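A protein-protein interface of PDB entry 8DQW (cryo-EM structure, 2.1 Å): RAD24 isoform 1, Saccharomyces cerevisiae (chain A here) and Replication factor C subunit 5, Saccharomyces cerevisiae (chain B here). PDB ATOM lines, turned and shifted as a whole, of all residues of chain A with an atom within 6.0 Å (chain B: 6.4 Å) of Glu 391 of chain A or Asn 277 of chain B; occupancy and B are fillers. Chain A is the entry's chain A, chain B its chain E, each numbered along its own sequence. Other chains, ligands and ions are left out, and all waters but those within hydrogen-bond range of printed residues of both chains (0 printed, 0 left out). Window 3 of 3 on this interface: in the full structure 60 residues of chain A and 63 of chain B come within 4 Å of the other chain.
ND2 of Asn 388 of chain A sits at hydrogen-bond distance from O of Glu 391 of chain A (3.3 Å). O of Asn 385 of chain A is in hydrogen-bond range of N of Gly 390 of chain A (2.9 Å).
Among the printed residues, pairs that only touch across the chains: Asn 385 of chain A with Val 276 of chain B (3.8 Å), Asn 385 of chain A with Ile 280 of chain B (3.6 Å), Gly 390 of chain A with Val 276 of chain B (3.8 Å), Glu 391 of chain A with Asn 277 of chain B (3.8 Å) and Phe 392 of chain A with Val 276 of chain B (3.4 Å).
Printed residues of chain B within 4 Å of Asn 385 of chain A: Val 276 and Ile 280. Glu 391 of chain A touches just one residue of chain B: Asn 277 (3.8 Å). Of the printed residues of chain A, Val 276 of chain B touches Asn 385 (3.8 Å), Gly 390 (3.8 Å) and Phe 392 (3.4 Å). Of chain A, only Glu 391 comes within 4 Å of Asn 277 of chain B. Of the printed residues of chain A, Ile 280 of chain B touches Asn 385. Cys 282 of chain B touches none of the printed residues of chain A. The nearest residue of chain A that does not touch Asn 277 of chain B is Gly 390 of chain A (4.03 Å).
Of the 8 printed residues of chain A, 4 touch a printed residue of chain B. Printed residues of chain B that touch a printed residue of chain A: Val 276, Asn 277 and Ile 280. Hydrophobic or aromatic side chains of chain B that line the printed part of chain A: Val 276 and Ile 280.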
ATOM      1  N   ASN A 385     -26.687 -23.603 -13.439  1.00  0.00           N
ATOM      2  CA  ASN A 385     -27.116 -24.114 -12.143  1.00  0.00           C
ATOM      3  C   ASN A 385     -28.473 -23.576 -11.711  1.00  0.00           C
ATOM      4  O   ASN A 385     -29.065 -24.123 -10.775  1.00  0.00           O
ATOM      5  CB  ASN A 385     -26.073 -23.778 -11.075  1.00  0.00           C
ATOM      6  CG  ASN A 385     -25.952 -22.289 -10.830  1.00  0.00           C
ATOM      7  OD1 ASN A 385     -25.429 -21.552 -11.664  1.00  0.00           O
ATOM      8  ND2 ASN A 385     -26.442 -21.835  -9.682  1.00  0.00           N
ATOM      9  N   PHE A 387     -31.170 -23.995 -13.077  1.00  0.00           N
ATOM     10  CA  PHE A 387     -32.202 -24.973 -13.396  1.00  0.00           C
ATOM     11  C   PHE A 387     -32.581 -25.756 -12.144  1.00  0.00           C
ATOM     12  O   PHE A 387     -31.728 -26.396 -11.520  1.00  0.00           O
ATOM     13  CB  PHE A 387     -31.710 -25.916 -14.490  1.00  0.00           C
ATOM     14  CG  PHE A 387     -32.776 -26.821 -15.034  1.00  0.00           C
ATOM     15  CD1 PHE A 387     -33.565 -26.423 -16.100  1.00  0.00           C
ATOM     16  CD2 PHE A 387     -32.988 -28.072 -14.480  1.00  0.00           C
ATOM     17  CE1 PHE A 387     -34.548 -27.254 -16.602  1.00  0.00           C
ATOM     18  CE2 PHE A 387     -33.969 -28.908 -14.978  1.00  0.00           C
ATOM     19  CZ  PHE A 387     -34.749 -28.499 -16.041  1.00  0.00           C
ATOM     20  N   ASN A 388     -33.864 -25.711 -11.783  1.00  0.00           N
ATOM     21  CA  ASN A 388     -34.372 -26.391 -10.593  1.00  0.00           C
ATOM     22  C   ASN A 388     -33.642 -25.934  -9.334  1.00  0.00           C
ATOM     23  O   ASN A 388     -33.516 -26.691  -8.368  1.00  0.00           O
ATOM     24  CB  ASN A 388     -34.276 -27.911 -10.740  1.00  0.00           C
ATOM     25  CG  ASN A 388     -35.325 -28.646  -9.925  1.00  0.00           C
ATOM     26  OD1 ASN A 388     -36.295 -28.051  -9.458  1.00  0.00           O
ATOM     27  ND2 ASN A 388     -35.134 -29.948  -9.753  1.00  0.00           N
ATOM     28  N   LYS A 389     -33.157 -24.692  -9.335  1.00  0.00           N
ATOM     29  CA  LYS A 389     -32.373 -24.161  -8.222  1.00  0.00           C
ATOM     30  C   LYS A 389     -31.225 -25.105  -7.870  1.00  0.00           C
ATOM     31  O   LYS A 389     -30.921 -25.349  -6.701  1.00  0.00           O
ATOM     32  CB  LYS A 389     -33.261 -23.894  -7.005  1.00  0.00           C
ATOM     33  CG  LYS A 389     -34.010 -22.577  -7.075  1.00  0.00           C
ATOM     34  CD  LYS A 389     -34.952 -22.402  -5.895  1.00  0.00           C
ATOM     35  CE  LYS A 389     -36.147 -21.541  -6.263  1.00  0.00           C
ATOM     36  NZ  LYS A 389     -36.678 -20.790  -5.091  1.00  0.00           N
ATOM     37  N   GLY A 390     -30.584 -25.645  -8.902  1.00  0.00           N
ATOM     38  CA  GLY A 390     -29.451 -26.535  -8.700  1.00  0.00           C
ATOM     39  C   GLY A 390     -29.799 -27.831  -8.001  1.00  0.00           C
ATOM     40  O   GLY A 390     -29.055 -28.273  -7.116  1.00  0.00           O
ATOM     41  N   GLU A 391     -30.912 -28.459  -8.383  1.00  0.00           N
ATOM     42  CA  GLU A 391     -31.324 -29.719  -7.776  1.00  0.00           C
ATOM     43  C   GLU A 391     -31.399 -30.826  -8.820  1.00  0.00           C
ATOM     44  O   GLU A 391     -32.379 -31.576  -8.869  1.00  0.00           O
ATOM     45  CB  GLU A 391     -32.677 -29.565  -7.074  1.00  0.00           C
ATOM     46  CG  GLU A 391     -32.690 -28.556  -5.930  1.00  0.00           C
ATOM     47  CD  GLU A 391     -31.506 -28.704  -4.992  1.00  0.00           C
ATOM     48  OE1 GLU A 391     -31.121 -29.854  -4.695  1.00  0.00           O
ATOM     49  OE2 GLU A 391     -30.964 -27.669  -4.552  1.00  0.00           O
ATOM     50  N   PHE A 392     -30.377 -30.929  -9.664  1.00  0.00           N
ATOM     51  CA  PHE A 392     -30.252 -32.010 -10.628  1.00  0.00           C
ATOM     52  C   PHE A 392     -28.925 -32.729 -10.413  1.00  0.00           C
ATOM     53  O   PHE A 392     -28.085 -32.310  -9.613  1.00  0.00           O
ATOM     54  CB  PHE A 392     -30.365 -31.493 -12.069  1.00  0.00           C
ATOM     55  CG  PHE A 392     -29.475 -30.320 -12.369  1.00  0.00           C
ATOM     56  CD1 PHE A 392     -29.882 -29.030 -12.070  1.00  0.00           C
ATOM     57  CD2 PHE A 392     -28.240 -30.508 -12.962  1.00  0.00           C
ATOM     58  CE1 PHE A 392     -29.067 -27.950 -12.350  1.00  0.00           C
ATOM     59  CE2 PHE A 392     -27.421 -29.433 -13.246  1.00  0.00           C
ATOM     60  CZ  PHE A 392     -27.834 -28.153 -12.940  1.00  0.00           C
ATOM     61  N   SER A 393     -28.746 -33.826 -11.141  1.00  0.00           N
ATOM     62  CA  SER A 393     -27.599 -34.694 -10.921  1.00  0.00           C
ATOM     63  C   SER A 393     -26.293 -33.984 -11.262  1.00  0.00           C
ATOM     64  O   SER A 393     -26.225 -33.156 -12.174  1.00  0.00           O
ATOM     65  CB  SER A 393     -27.728 -35.966 -11.759  1.00  0.00           C
ATOM     66  OG  SER A 393     -26.630 -36.835 -11.541  1.00  0.00           O
ATOM     67  N   LYS B 269     -13.542 -29.578   1.092  1.00  0.00           N
ATOM     68  CA  LYS B 269     -14.935 -29.335   0.731  1.00  0.00           C
ATOM     69  C   LYS B 269     -15.376 -30.245  -0.409  1.00  0.00           C
ATOM     70  O   LYS B 269     -16.475 -30.809  -0.374  1.00  0.00           O
ATOM     71  CB  LYS B 269     -15.125 -27.867   0.350  1.00  0.00           C
ATOM     72  CG  LYS B 269     -16.334 -27.606  -0.535  1.00  0.00           C
ATOM     73  CD  LYS B 269     -16.810 -26.173  -0.411  1.00  0.00           C
ATOM     74  CE  LYS B 269     -18.209 -26.000  -0.974  1.00  0.00           C
ATOM     75  NZ  LYS B 269     -19.249 -26.644  -0.123  1.00  0.00           N
ATOM     76  N   SER B 275     -22.136 -31.948  -5.061  1.00  0.00           N
ATOM     77  CA  SER B 275     -23.432 -31.515  -5.568  1.00  0.00           C
ATOM     78  C   SER B 275     -23.231 -30.247  -6.387  1.00  0.00           C
ATOM     79  O   SER B 275     -22.135 -29.684  -6.441  1.00  0.00           O
ATOM     80  CB  SER B 275     -24.429 -31.281  -4.429  1.00  0.00           C
ATOM     81  OG  SER B 275     -24.114 -30.101  -3.712  1.00  0.00           O
ATOM     82  N   VAL B 276     -24.315 -29.804  -7.030  1.00  0.00           N
ATOM     83  CA  VAL B 276     -24.240 -28.627  -7.891  1.00  0.00           C
ATOM     84  C   VAL B 276     -23.868 -27.393  -7.077  1.00  0.00           C
ATOM     85  O   VAL B 276     -22.988 -26.613  -7.464  1.00  0.00           O
ATOM     86  CB  VAL B 276     -25.571 -28.427  -8.639  1.00  0.00           C
ATOM     87  CG1 VAL B 276     -25.515 -27.176  -9.507  1.00  0.00           C
ATOM     88  CG2 VAL B 276     -25.897 -29.651  -9.484  1.00  0.00           C
ATOM     89  N   ASN B 277     -24.528 -27.198  -5.932  1.00  0.00           N
ATOM     90  CA  ASN B 277     -24.238 -26.031  -5.102  1.00  0.00           C
ATOM     91  C   ASN B 277     -22.796 -26.051  -4.613  1.00  0.00           C
ATOM     92  O   ASN B 277     -22.127 -25.008  -4.577  1.00  0.00           O
ATOM     93  CB  ASN B 277     -25.206 -25.979  -3.919  1.00  0.00           C
ATOM     94  CG  ASN B 277     -26.649 -25.845  -4.354  1.00  0.00           C
ATOM     95  OD1 ASN B 277     -26.941 -25.291  -5.415  1.00  0.00           O
ATOM     96  ND2 ASN B 277     -27.564 -26.349  -3.534  1.00  0.00           N
ATOM     97  N   SER B 278     -22.308 -27.226  -4.213  1.00  0.00           N
ATOM     98  CA  SER B 278     -20.898 -27.359  -3.873  1.00  0.00           C
ATOM     99  C   SER B 278     -20.021 -26.908  -5.033  1.00  0.00           C
ATOM    100  O   SER B 278     -19.004 -26.237  -4.830  1.00  0.00           O
ATOM    101  CB  SER B 278     -20.590 -28.808  -3.490  1.00  0.00           C
ATOM    102  OG  SER B 278     -19.329 -28.914  -2.852  1.00  0.00           O
ATOM    103  N   LEU B 279     -20.413 -27.252  -6.261  1.00  0.00           N
ATOM    104  CA  LEU B 279     -19.643 -26.840  -7.430  1.00  0.00           C
ATOM    105  C   LEU B 279     -19.664 -25.324  -7.603  1.00  0.00           C
ATOM    106  O   LEU B 279     -18.656 -24.727  -7.994  1.00  0.00           O
ATOM    107  CB  LEU B 279     -20.183 -27.537  -8.680  1.00  0.00           C
ATOM    108  CG  LEU B 279     -19.372 -27.348  -9.963  1.00  0.00           C
ATOM    109  CD1 LEU B 279     -18.039 -28.067  -9.860  1.00  0.00           C
ATOM    110  CD2 LEU B 279     -20.152 -27.846 -11.169  1.00  0.00           C
ATOM    111  N   ILE B 280     -20.801 -24.683  -7.327  1.00  0.00           N
ATOM    112  CA  ILE B 280     -20.869 -23.227  -7.453  1.00  0.00           C
ATOM    113  C   ILE B 280     -19.962 -22.559  -6.421  1.00  0.00           C
ATOM    114  O   ILE B 280     -19.255 -21.587  -6.724  1.00  0.00           O
ATOM    115  CB  ILE B 280     -22.325 -22.734  -7.327  1.00  0.00           C
ATOM    116  CG1 ILE B 280     -23.305 -23.643  -8.082  1.00  0.00           C
ATOM    117  CG2 ILE B 280     -22.447 -21.310  -7.844  1.00  0.00           C
ATOM    118  CD1 ILE B 280     -22.832 -24.118  -9.455  1.00  0.00           C
ATOM    119  N   GLU B 281     -19.966 -23.063  -5.185  1.00  0.00           N
ATOM    120  CA  GLU B 281     -19.057 -22.508  -4.183  1.00  0.00           C
ATOM    121  C   GLU B 281     -17.598 -22.754  -4.564  1.00  0.00           C
ATOM    122  O   GLU B 281     -16.727 -21.906  -4.318  1.00  0.00           O
ATOM    123  CB  GLU B 281     -19.362 -23.087  -2.801  1.00  0.00           C
ATOM    124  CG  GLU B 281     -20.840 -23.156  -2.458  1.00  0.00           C
ATOM    125  CD  GLU B 281     -21.089 -23.197  -0.963  1.00  0.00           C
ATOM    126  OE1 GLU B 281     -20.765 -22.204  -0.279  1.00  0.00           O
ATOM    127  OE2 GLU B 281     -21.609 -24.222  -0.476  1.00  0.00           O
ATOM    128  N   CYS B 282     -17.310 -23.913  -5.164  1.00  0.00           N
ATOM    129  CA  CYS B 282     -15.960 -24.170  -5.652  1.00  0.00           C
ATOM    130  C   CYS B 282     -15.575 -23.173  -6.738  1.00  0.00           C
ATOM    131  O   CYS B 282     -14.431 -22.712  -6.791  1.00  0.00           O
ATOM    132  CB  CYS B 282     -15.858 -25.603  -6.173  1.00  0.00           C
ATOM    133  SG  CYS B 282     -15.773 -26.862  -4.877  1.00  0.00           S
